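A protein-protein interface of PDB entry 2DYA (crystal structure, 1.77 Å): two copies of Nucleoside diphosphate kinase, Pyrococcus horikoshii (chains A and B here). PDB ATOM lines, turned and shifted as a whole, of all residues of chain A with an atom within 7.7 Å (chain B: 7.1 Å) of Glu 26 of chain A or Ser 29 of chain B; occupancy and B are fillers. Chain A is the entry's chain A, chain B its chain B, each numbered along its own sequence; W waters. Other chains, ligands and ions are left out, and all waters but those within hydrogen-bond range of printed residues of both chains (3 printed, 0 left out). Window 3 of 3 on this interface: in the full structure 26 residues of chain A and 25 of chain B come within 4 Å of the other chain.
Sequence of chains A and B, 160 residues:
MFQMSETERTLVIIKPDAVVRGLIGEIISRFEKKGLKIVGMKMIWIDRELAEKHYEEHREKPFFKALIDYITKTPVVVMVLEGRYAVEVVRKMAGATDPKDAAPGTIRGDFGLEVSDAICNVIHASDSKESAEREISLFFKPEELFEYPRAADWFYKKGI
OE2 of Glu 32 of chain B lies within hydrogen-bond range of N of Ile 24 of chain A (3.0 Å). O of Gly 25 of chain A lies close to O of Gly 25 of chain B, 3.4 Å away. The backbone NH (N) of Leu 23 of chain B sits at hydrogen-bond distance from the side-chain carboxylate (OE2) of Glu 32 of chain A (3.3 Å). The backbone NH (N) of Gly 25 of chain A is in hydrogen-bond range of the side-chain carboxylate (OE1) of Glu 32 of chain B (2.8 Å). The side-chain hydroxyl (OG) of Ser 29 of chain A sits at hydrogen-bond distance from the backbone NH (N) of Glu 26 of chain B (3.0 Å). O of Gly 22 of chain A sits close to OE2 of Glu 32 of chain B (3.4 Å). The backbone NH (N) of Leu 23 of chain A sits at hydrogen-bond distance from the side-chain carboxylate (OE2) of Glu 32 of chain B (3.3 Å). OE2 of Glu 32 of chain A is in hydrogen-bond range of N of Ile 24 of chain B (2.9 Å). The side-chain carboxylate of Glu 32 of chain A is in hydrogen-bond range of the backbone NH of Gly 25 of chain B, 2.7 Å away. OG of Ser 29 of chain B is in hydrogen-bond range of N of Glu 26 of chain A, 3.0 Å away.
The side-chain hydroxyl (OG) of Ser 29 of chain B lies within hydrogen-bond range of the backbone carbonyl oxygen (O) of Gly 25 of chain B. O of Gly 25 of chain A is in hydrogen-bond range of OG of Ser 29 of chain A, at 3.0 Å.
Among the printed residues, pairs that only touch across the chains: Gly 25 of chain A with Ile 28 of chain B (3.7 Å), Gly 25 of chain A with Ser 29 of chain B (3.1 Å), Ile 28 of chain A with Gly 25 of chain B (3.7 Å), Ile 28 of chain A with Ile 28 of chain B (3.7 Å) and Ser 29 of chain A with Gly 25 of chain B (3.1 Å).
Glu 26 of chain A touches just one residue of chain B: Ser 29 (3.0 Å). Gly 25 of chain A touches just these residues of chain B: Gly 25 (3.2 Å), Ile 28 (3.7 Å), Ser 29 (3.1 Å) and Glu 32 (2.8 Å). Printed residues of chain B within 4 Å of Ser 29 of chain A: Gly 25 (3.1 Å) and Glu 26 (3.0 Å). Of the printed residues of chain B, Leu 23 of chain A touches Glu 32 (3.3 Å). Of the printed residues of chain A, Ile 24 of chain B touches Glu 32. Of the printed residues of chain A, Ile 28 of chain B touches Gly 25 and Ile 28. Arg 30 of chain A touches none of the printed residues of chain B. Met 93 of chain B touches none of the printed residues of chain A. The nearest residue of chain A that does not touch Ser 29 of chain B is Ser 29 of chain A (5.0 Å). The nearest printed residue of chain A that does not touch Gly 25 of chain B is Glu 26 of chain A (4.5 Å).
Of the 15 printed residues of chain A, 8 touch a printed residue of chain B. Hydrophobic or aromatic side chains of chain A within 4 Å of the printed part of chain B: Ile 24 and Ile 28. Of the 15 printed residues of chain B, 7 touch a printed residue of chain A. Hydrophobic or aromatic side chains of chain B that line the printed part of chain A: Ile 24 and Ile 28.
Ile 24 of chain A touches Glu 32 of chain B, and with the chains exchanged Glu 32 of chain A touches Ile 24 of chain B. Gly 25 of chain A touches its own counterpart, Gly 25 of chain B. Gly 25 of chain A touches Ser 29 of chain B, and with the chains exchanged Ser 29 of chain A touches Gly 25 of chain B. Glu 26 of chain A touches Ser 29 of chain B, and with the chains exchanged Ser 29 of chain A touches Glu 26 of chain B. 10 positions are printed for both chains.
Water W2 lies within hydrogen-bond range of the side-chain carboxylate of Glu 32 of chain B, the side-chain hydroxyl of Ser 29 of chain B, the backbone NH of Glu 26 of chain A, the backbone carbonyl oxygen of Gly 22 of chain A and the backbone NH of Gly 25 of chain A. Water W1 lies within hydrogen-bond range of the side-chain hydroxyl (OG) of Ser 29 of chain A (2.7 Å), the side-chain hydroxyl (OG) of Ser 29 of chain B (2.8 Å), the backbone carbonyl oxygen (O) of Gly 25 of chain A (3.2 Å) and the backbone carbonyl oxygen (O) of Gly 25 of chain B (3.4 Å). Water W3 lies within hydrogen-bond range of the side-chain hydroxyl (OG) of Ser 29 of chain A (2.8 Å), the side-chain carboxylate (OE1) of Glu 32 of chain A (2.8 Å), the backbone NH (N) of Glu 26 of chain B (3.0 Å) and the backbone NH (N) of Gly 25 of chain B (3.3 Å).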
ATOM      1  N   ILE A  14      20.924   0.734  -6.844  1.00  0.00           N
ATOM      2  CA  ILE A  14      20.023   0.746  -7.986  1.00  0.00           C
ATOM      3  C   ILE A  14      20.756   1.703  -8.928  1.00  0.00           C
ATOM      4  O   ILE A  14      20.774   2.916  -8.715  1.00  0.00           O
ATOM      5  CB  ILE A  14      18.635   1.293  -7.592  1.00  0.00           C
ATOM      6  CG1 ILE A  14      17.987   0.338  -6.577  1.00  0.00           C
ATOM      7  CG2 ILE A  14      17.765   1.456  -8.834  1.00  0.00           C
ATOM      8  CD1 ILE A  14      16.679   0.825  -5.976  1.00  0.00           C
ATOM      9  N   ARG A  21      15.220   4.680 -16.178  1.00  0.00           N
ATOM     10  CA  ARG A  21      14.087   3.935 -16.718  1.00  0.00           C
ATOM     11  C   ARG A  21      12.877   3.845 -15.771  1.00  0.00           C
ATOM     12  O   ARG A  21      11.859   3.261 -16.125  1.00  0.00           O
ATOM     13  CB  ARG A  21      14.543   2.527 -17.111  1.00  0.00           C
ATOM     14  CG  ARG A  21      15.540   2.502 -18.263  1.00  0.00           C
ATOM     15  CD  ARG A  21      16.200   1.138 -18.397  1.00  0.00           C
ATOM     16  NE  ARG A  21      15.237   0.087 -18.704  1.00  0.00           N
ATOM     17  CZ  ARG A  21      15.490  -1.214 -18.597  1.00  0.00           C
ATOM     18  NH1 ARG A  21      16.683  -1.633 -18.189  1.00  0.00           N
ATOM     19  NH2 ARG A  21      14.543  -2.095 -18.894  1.00  0.00           N
ATOM     20  N   GLY A  22      12.993   4.418 -14.575  1.00  0.00           N
ATOM     21  CA  GLY A  22      11.894   4.386 -13.620  1.00  0.00           C
ATOM     22  C   GLY A  22      11.591   3.015 -13.030  1.00  0.00           C
ATOM     23  O   GLY A  22      10.423   2.643 -12.873  1.00  0.00           O
ATOM     24  N   LEU A  23      12.635   2.267 -12.681  1.00  0.00           N
ATOM     25  CA  LEU A  23      12.467   0.928 -12.118  1.00  0.00           C
ATOM     26  C   LEU A  23      12.777   0.816 -10.626  1.00  0.00           C
ATOM     27  O   LEU A  23      12.763  -0.286 -10.076  1.00  0.00           O
ATOM     28  CB  LEU A  23      13.353  -0.068 -12.867  1.00  0.00           C
ATOM     29  CG  LEU A  23      13.142  -0.170 -14.372  1.00  0.00           C
ATOM     30  CD1 LEU A  23      14.108  -1.200 -14.933  1.00  0.00           C
ATOM     31  CD2 LEU A  23      11.702  -0.543 -14.671  1.00  0.00           C
ATOM     32  N   ILE A  24      13.059   1.942  -9.977  1.00  0.00           N
ATOM     33  CA  ILE A  24      13.381   1.950  -8.547  1.00  0.00           C
ATOM     34  C   ILE A  24      12.344   1.219  -7.694  1.00  0.00           C
ATOM     35  O   ILE A  24      12.690   0.345  -6.897  1.00  0.00           O
ATOM     36  CB  ILE A  24      13.508   3.400  -8.008  1.00  0.00           C
ATOM     37  CG1 ILE A  24      14.618   4.141  -8.761  1.00  0.00           C
ATOM     38  CG2 ILE A  24      13.791   3.383  -6.504  1.00  0.00           C
ATOM     39  CD1 ILE A  24      14.757   5.609  -8.379  1.00  0.00           C
ATOM     40  N   GLY A  25      11.075   1.586  -7.857  1.00  0.00           N
ATOM     41  CA  GLY A  25      10.014   0.967  -7.080  1.00  0.00           C
ATOM     42  C   GLY A  25       9.843  -0.527  -7.301  1.00  0.00           C
ATOM     43  O   GLY A  25       9.630  -1.284  -6.346  1.00  0.00           O
ATOM     44  N   GLU A  26       9.938  -0.957  -8.559  1.00  0.00           N
ATOM     45  CA  GLU A  26       9.785  -2.366  -8.904  1.00  0.00           C
ATOM     46  C   GLU A  26      10.898  -3.204  -8.275  1.00  0.00           C
ATOM     47  O   GLU A  26      10.647  -4.280  -7.734  1.00  0.00           O
ATOM     48  CB  GLU A  26       9.782  -2.525 -10.429  1.00  0.00           C
ATOM     49  CG  GLU A  26       8.845  -1.536 -11.112  1.00  0.00           C
ATOM     50  CD  GLU A  26       8.770  -1.703 -12.614  1.00  0.00           C
ATOM     51  OE1 GLU A  26       8.407  -0.723 -13.294  1.00  0.00           O
ATOM     52  OE2 GLU A  26       9.057  -2.810 -13.111  1.00  0.00           O
ATOM     53  N   ILE A  27      12.126  -2.696  -8.335  1.00  0.00           N
ATOM     54  CA  ILE A  27      13.267  -3.384  -7.752  1.00  0.00           C
ATOM     55  C   ILE A  27      13.094  -3.476  -6.232  1.00  0.00           C
ATOM     56  O   ILE A  27      13.255  -4.546  -5.649  1.00  0.00           O
ATOM     57  CB  ILE A  27      14.573  -2.643  -8.079  1.00  0.00           C
ATOM     58  CG1 ILE A  27      14.807  -2.670  -9.589  1.00  0.00           C
ATOM     59  CG2 ILE A  27      15.737  -3.279  -7.331  1.00  0.00           C
ATOM     60  CD1 ILE A  27      15.954  -1.787 -10.066  1.00  0.00           C
ATOM     61  N   ILE A  28      12.756  -2.355  -5.599  1.00  0.00           N
ATOM     62  CA  ILE A  28      12.555  -2.334  -4.149  1.00  0.00           C
ATOM     63  C   ILE A  28      11.463  -3.322  -3.731  1.00  0.00           C
ATOM     64  O   ILE A  28      11.598  -4.014  -2.727  1.00  0.00           O
ATOM     65  CB  ILE A  28      12.151  -0.920  -3.644  1.00  0.00           C
ATOM     66  CG1 ILE A  28      13.337   0.037  -3.752  1.00  0.00           C
ATOM     67  CG2 ILE A  28      11.673  -0.994  -2.196  1.00  0.00           C
ATOM     68  CD1 ILE A  28      13.009   1.454  -3.337  1.00  0.00           C
ATOM     69  N   SER A  29      10.382  -3.383  -4.501  1.00  0.00           N
ATOM     70  CA  SER A  29       9.278  -4.279  -4.174  1.00  0.00           C
ATOM     71  C   SER A  29       9.698  -5.745  -4.157  1.00  0.00           C
ATOM     72  O   SER A  29       9.204  -6.526  -3.340  1.00  0.00           O
ATOM     73  CB  SER A  29       8.116  -4.076  -5.154  1.00  0.00           C
ATOM     74  OG  SER A  29       7.478  -2.837  -4.925  1.00  0.00           O
ATOM     75  N   ARG A  30      10.606  -6.124  -5.050  1.00  0.00           N
ATOM     76  CA  ARG A  30      11.061  -7.510  -5.091  1.00  0.00           C
ATOM     77  C   ARG A  30      11.693  -7.907  -3.759  1.00  0.00           C
ATOM     78  O   ARG A  30      11.493  -9.016  -3.270  1.00  0.00           O
ATOM     79  CB  ARG A  30      12.059  -7.717  -6.232  1.00  0.00           C
ATOM     80  CG  ARG A  30      11.445  -7.465  -7.591  1.00  0.00           C
ATOM     81  CD  ARG A  30      12.144  -8.231  -8.681  1.00  0.00           C
ATOM     82  NE  ARG A  30      11.425  -8.116  -9.946  1.00  0.00           N
ATOM     83  CZ  ARG A  30      11.686  -8.852 -11.021  1.00  0.00           C
ATOM     84  NH1 ARG A  30      12.650  -9.760 -10.984  1.00  0.00           N
ATOM     85  NH2 ARG A  30      10.981  -8.684 -12.133  1.00  0.00           N
ATOM     86  N   PHE A  31      12.447  -6.989  -3.170  1.00  0.00           N
ATOM     87  CA  PHE A  31      13.089  -7.259  -1.895  1.00  0.00           C
ATOM     88  C   PHE A  31      12.064  -7.276  -0.764  1.00  0.00           C
ATOM     89  O   PHE A  31      12.079  -8.174   0.079  1.00  0.00           O
ATOM     90  CB  PHE A  31      14.177  -6.217  -1.630  1.00  0.00           C
ATOM     91  CG  PHE A  31      15.270  -6.224  -2.660  1.00  0.00           C
ATOM     92  CD1 PHE A  31      15.895  -7.420  -3.017  1.00  0.00           C
ATOM     93  CD2 PHE A  31      15.673  -5.042  -3.278  1.00  0.00           C
ATOM     94  CE1 PHE A  31      16.906  -7.443  -3.979  1.00  0.00           C
ATOM     95  CE2 PHE A  31      16.685  -5.052  -4.242  1.00  0.00           C
ATOM     96  CZ  PHE A  31      17.301  -6.256  -4.593  1.00  0.00           C
ATOM     97  N   GLU A  32      11.170  -6.293  -0.749  1.00  0.00           N
ATOM     98  CA  GLU A  32      10.138  -6.240   0.280  1.00  0.00           C
ATOM     99  C   GLU A  32       9.271  -7.498   0.252  1.00  0.00           C
ATOM    100  O   GLU A  32       8.933  -8.048   1.298  1.00  0.00           O
ATOM    101  CB  GLU A  32       9.257  -5.007   0.085  1.00  0.00           C
ATOM    102  CG  GLU A  32       9.944  -3.696   0.421  1.00  0.00           C
ATOM    103  CD  GLU A  32       9.071  -2.500   0.117  1.00  0.00           C
ATOM    104  OE1 GLU A  32       8.830  -2.232  -1.076  1.00  0.00           O
ATOM    105  OE2 GLU A  32       8.621  -1.835   1.071  1.00  0.00           O
ATOM    106  N   ILE A 107      16.293 -10.107 -11.288  1.00  0.00           N
ATOM    107  CA  ILE A 107      16.179  -8.688 -11.595  1.00  0.00           C
ATOM    108  C   ILE A 107      16.903  -8.331 -12.904  1.00  0.00           C
ATOM    109  O   ILE A 107      16.327  -7.679 -13.776  1.00  0.00           O
ATOM    110  CB  ILE A 107      16.710  -7.846 -10.413  1.00  0.00           C
ATOM    111  CG1 ILE A 107      15.774  -8.035  -9.209  1.00  0.00           C
ATOM    112  CG2 ILE A 107      16.831  -6.376 -10.815  1.00  0.00           C
ATOM    113  CD1 ILE A 107      16.344  -7.571  -7.891  1.00  0.00           C
ATOM    114  N   PHE A 111      14.855  -7.245 -16.255  1.00  0.00           N
ATOM    115  CA  PHE A 111      15.012  -5.835 -16.618  1.00  0.00           C
ATOM    116  C   PHE A 111      16.226  -5.418 -17.454  1.00  0.00           C
ATOM    117  O   PHE A 111      16.202  -4.356 -18.077  1.00  0.00           O
ATOM    118  CB  PHE A 111      15.009  -4.961 -15.353  1.00  0.00           C
ATOM    119  CG  PHE A 111      13.791  -5.126 -14.487  1.00  0.00           C
ATOM    120  CD1 PHE A 111      12.522  -5.216 -15.045  1.00  0.00           C
ATOM    121  CD2 PHE A 111      13.913  -5.143 -13.099  1.00  0.00           C
ATOM    122  CE1 PHE A 111      11.387  -5.319 -14.229  1.00  0.00           C
ATOM    123  CE2 PHE A 111      12.788  -5.243 -12.277  1.00  0.00           C
ATOM    124  CZ  PHE A 111      11.526  -5.332 -12.843  1.00  0.00           C
ATOM    125  N   LEU B  23       5.356  -1.712   1.591  1.00  0.00           N
ATOM    126  CA  LEU B  23       4.708  -1.096   0.439  1.00  0.00           C
ATOM    127  C   LEU B  23       5.511   0.028  -0.213  1.00  0.00           C
ATOM    128  O   LEU B  23       5.019   0.685  -1.127  1.00  0.00           O
ATOM    129  CB  LEU B  23       3.338  -0.546   0.851  1.00  0.00           C
ATOM    130  CG  LEU B  23       2.298  -1.559   1.334  1.00  0.00           C
ATOM    131  CD1 LEU B  23       1.053  -0.818   1.810  1.00  0.00           C
ATOM    132  CD2 LEU B  23       1.959  -2.530   0.206  1.00  0.00           C
ATOM    133  N   ILE B  24       6.737   0.247   0.251  1.00  0.00           N
ATOM    134  CA  ILE B  24       7.580   1.313  -0.287  1.00  0.00           C
ATOM    135  C   ILE B  24       7.726   1.267  -1.804  1.00  0.00           C
ATOM    136  O   ILE B  24       7.504   2.274  -2.485  1.00  0.00           O
ATOM    137  CB  ILE B  24       8.999   1.277   0.322  1.00  0.00           C
ATOM    138  CG1 ILE B  24       8.932   1.542   1.829  1.00  0.00           C
ATOM    139  CG2 ILE B  24       9.879   2.315  -0.366  1.00  0.00           C
ATOM    140  CD1 ILE B  24      10.259   1.344   2.539  1.00  0.00           C
ATOM    141  N   GLY B  25       8.110   0.101  -2.317  1.00  0.00           N
ATOM    142  CA  GLY B  25       8.299  -0.067  -3.747  1.00  0.00           C
ATOM    143  C   GLY B  25       7.053   0.172  -4.576  1.00  0.00           C
ATOM    144  O   GLY B  25       7.112   0.868  -5.588  1.00  0.00           O
ATOM    145  N   GLU B  26       5.929  -0.407  -4.158  1.00  0.00           N
ATOM    146  CA  GLU B  26       4.671  -0.247  -4.881  1.00  0.00           C
ATOM    147  C   GLU B  26       4.271   1.225  -4.986  1.00  0.00           C
ATOM    148  O   GLU B  26       3.802   1.673  -6.030  1.00  0.00           O
ATOM    149  CB  GLU B  26       3.568  -1.063  -4.195  1.00  0.00           C
ATOM    150  CG  GLU B  26       3.812  -2.570  -4.255  1.00  0.00           C
ATOM    151  CD  GLU B  26       2.952  -3.362  -3.278  1.00  0.00           C
ATOM    152  OE1 GLU B  26       1.714  -3.388  -3.441  1.00  0.00           O
ATOM    153  OE2 GLU B  26       3.522  -3.963  -2.341  1.00  0.00           O
ATOM    154  N   ILE B  27       4.467   1.979  -3.909  1.00  0.00           N
ATOM    155  CA  ILE B  27       4.135   3.404  -3.913  1.00  0.00           C
ATOM    156  C   ILE B  27       5.054   4.180  -4.869  1.00  0.00           C
ATOM    157  O   ILE B  27       4.577   4.971  -5.690  1.00  0.00           O
ATOM    158  CB  ILE B  27       4.230   4.000  -2.489  1.00  0.00           C
ATOM    159  CG1 ILE B  27       3.150   3.368  -1.600  1.00  0.00           C
ATOM    160  CG2 ILE B  27       4.069   5.513  -2.537  1.00  0.00           C
ATOM    161  CD1 ILE B  27       3.185   3.814  -0.149  1.00  0.00           C
ATOM    162  N   ILE B  28       6.361   3.942  -4.777  1.00  0.00           N
ATOM    163  CA  ILE B  28       7.321   4.619  -5.652  1.00  0.00           C
ATOM    164  C   ILE B  28       7.020   4.335  -7.133  1.00  0.00           C
ATOM    165  O   ILE B  28       7.064   5.240  -7.964  1.00  0.00           O
ATOM    166  CB  ILE B  28       8.781   4.183  -5.340  1.00  0.00           C
ATOM    167  CG1 ILE B  28       9.196   4.704  -3.961  1.00  0.00           C
ATOM    168  CG2 ILE B  28       9.730   4.716  -6.409  1.00  0.00           C
ATOM    169  CD1 ILE B  28      10.498   4.121  -3.442  1.00  0.00           C
ATOM    170  N   SER B  29       6.704   3.083  -7.455  1.00  0.00           N
ATOM    171  CA  SER B  29       6.400   2.713  -8.833  1.00  0.00           C
ATOM    172  C   SER B  29       5.221   3.497  -9.403  1.00  0.00           C
ATOM    173  O   SER B  29       5.208   3.825 -10.588  1.00  0.00           O
ATOM    174  CB  SER B  29       6.107   1.213  -8.938  1.00  0.00           C
ATOM    175  OG  SER B  29       7.272   0.447  -8.690  1.00  0.00           O
ATOM    176  N   ARG B  30       4.224   3.795  -8.574  1.00  0.00           N
ATOM    177  CA  ARG B  30       3.074   4.546  -9.068  1.00  0.00           C
ATOM    178  C   ARG B  30       3.473   5.928  -9.570  1.00  0.00           C
ATOM    179  O   ARG B  30       2.942   6.409 -10.567  1.00  0.00           O
ATOM    180  CB  ARG B  30       2.007   4.672  -7.982  1.00  0.00           C
ATOM    181  CG  ARG B  30       1.361   3.346  -7.652  1.00  0.00           C
ATOM    182  CD  ARG B  30       0.080   3.540  -6.890  1.00  0.00           C
ATOM    183  NE  ARG B  30      -0.581   2.269  -6.622  1.00  0.00           N
ATOM    184  CZ  ARG B  30      -1.875   2.150  -6.351  1.00  0.00           C
ATOM    185  NH1 ARG B  30      -2.646   3.226  -6.313  1.00  0.00           N
ATOM    186  NH2 ARG B  30      -2.395   0.953  -6.125  1.00  0.00           N
ATOM    187  N   PHE B  31       4.413   6.562  -8.877  1.00  0.00           N
ATOM    188  CA  PHE B  31       4.886   7.882  -9.275  1.00  0.00           C
ATOM    189  C   PHE B  31       5.775   7.758 -10.512  1.00  0.00           C
ATOM    190  O   PHE B  31       5.625   8.512 -11.474  1.00  0.00           O
ATOM    191  CB  PHE B  31       5.668   8.536  -8.131  1.00  0.00           C
ATOM    192  CG  PHE B  31       4.850   8.746  -6.886  1.00  0.00           C
ATOM    193  CD1 PHE B  31       3.604   9.358  -6.957  1.00  0.00           C
ATOM    194  CD2 PHE B  31       5.334   8.345  -5.642  1.00  0.00           C
ATOM    195  CE1 PHE B  31       2.842   9.572  -5.801  1.00  0.00           C
ATOM    196  CE2 PHE B  31       4.583   8.553  -4.481  1.00  0.00           C
ATOM    197  CZ  PHE B  31       3.336   9.167  -4.563  1.00  0.00           C
ATOM    198  N   GLU B  32       6.698   6.800 -10.491  1.00  0.00           N
ATOM    199  CA  GLU B  32       7.579   6.606 -11.634  1.00  0.00           C
ATOM    200  C   GLU B  32       6.750   6.346 -12.885  1.00  0.00           C
ATOM    201  O   GLU B  32       7.015   6.914 -13.935  1.00  0.00           O
ATOM    202  CB  GLU B  32       8.528   5.434 -11.389  1.00  0.00           C
ATOM    203  CG  GLU B  32       9.651   5.736 -10.404  1.00  0.00           C
ATOM    204  CD  GLU B  32      10.524   4.524 -10.136  1.00  0.00           C
ATOM    205  OE1 GLU B  32       9.999   3.519  -9.604  1.00  0.00           O
ATOM    206  OE2 GLU B  32      11.729   4.579 -10.459  1.00  0.00           O
ATOM    207  N   LYS B  33       5.735   5.500 -12.758  1.00  0.00           N
ATOM    208  CA  LYS B  33       4.870   5.151 -13.880  1.00  0.00           C
ATOM    209  C   LYS B  33       4.081   6.353 -14.400  1.00  0.00           C
ATOM    210  O   LYS B  33       3.826   6.464 -15.600  1.00  0.00           O
ATOM    211  CB  LYS B  33       3.917   4.028 -13.463  1.00  0.00           C
ATOM    212  CG  LYS B  33       3.051   3.490 -14.591  1.00  0.00           C
ATOM    213  CD  LYS B  33       3.890   2.935 -15.742  1.00  0.00           C
ATOM    214  CE  LYS B  33       4.723   1.732 -15.313  1.00  0.00           C
ATOM    215  NZ  LYS B  33       3.865   0.639 -14.774  1.00  0.00           N
ATOM    216  N   LYS B  34       3.704   7.251 -13.494  1.00  0.00           N
ATOM    217  CA  LYS B  34       2.956   8.459 -13.842  1.00  0.00           C
ATOM    218  C   LYS B  34       3.832   9.415 -14.662  1.00  0.00           C
ATOM    219  O   LYS B  34       3.326  10.246 -15.424  1.00  0.00           O
ATOM    220  CB  LYS B  34       2.486   9.153 -12.558  1.00  0.00           C
ATOM    221  CG  LYS B  34       1.725  10.455 -12.754  1.00  0.00           C
ATOM    222  CD  LYS B  34       0.361  10.229 -13.372  1.00  0.00           C
ATOM    223  CE  LYS B  34      -0.472  11.503 -13.338  1.00  0.00           C
ATOM    224  NZ  LYS B  34      -1.811  11.327 -13.958  1.00  0.00           N
ATOM    225  N   GLY B  35       5.147   9.284 -14.495  1.00  0.00           N
ATOM    226  CA  GLY B  35       6.080  10.136 -15.204  1.00  0.00           C
ATOM    227  C   GLY B  35       6.750  11.141 -14.284  1.00  0.00           C
ATOM    228  O   GLY B  35       7.510  11.997 -14.740  1.00  0.00           O
ATOM    229  N   ILE B  38      11.913  11.452  -9.394  1.00  0.00           N
ATOM    230  CA  ILE B  38      12.374  11.444  -8.009  1.00  0.00           C
ATOM    231  C   ILE B  38      13.698  12.216  -7.959  1.00  0.00           C
ATOM    232  O   ILE B  38      14.735  11.702  -8.382  1.00  0.00           O
ATOM    233  CB  ILE B  38      12.619  10.000  -7.507  1.00  0.00           C
ATOM    234  CG1 ILE B  38      11.332   9.184  -7.622  1.00  0.00           C
ATOM    235  CG2 ILE B  38      13.101  10.022  -6.067  1.00  0.00           C
ATOM    236  CD1 ILE B  38      11.510   7.709  -7.320  1.00  0.00           C
ATOM    237  N   MET B  93      -3.454  11.543  -6.595  1.00  0.00           N
ATOM    238  CA  MET B  93      -3.007  10.155  -6.547  1.00  0.00           C
ATOM    239  C   MET B  93      -3.120   9.591  -5.128  1.00  0.00           C
ATOM    240  O   MET B  93      -3.416   8.412  -4.944  1.00  0.00           O
ATOM    241  CB  MET B  93      -1.556  10.046  -7.032  1.00  0.00           C
ATOM    242  CG  MET B  93      -1.358  10.373  -8.512  1.00  0.00           C
ATOM    243  SD  MET B  93       0.374  10.247  -9.018  1.00  0.00           S
ATOM    244  CE  MET B  93       0.608   8.461  -8.911  1.00  0.00           C
HETATM  245  O   HOH W   1       6.630  -1.972  -7.372  1.00  0.00           O
HETATM  246  O   HOH W   2       9.220   1.207 -10.488  1.00  0.00           O
HETATM  247  O   HOH W   3       6.347  -2.710  -2.348  1.00  0.00           O
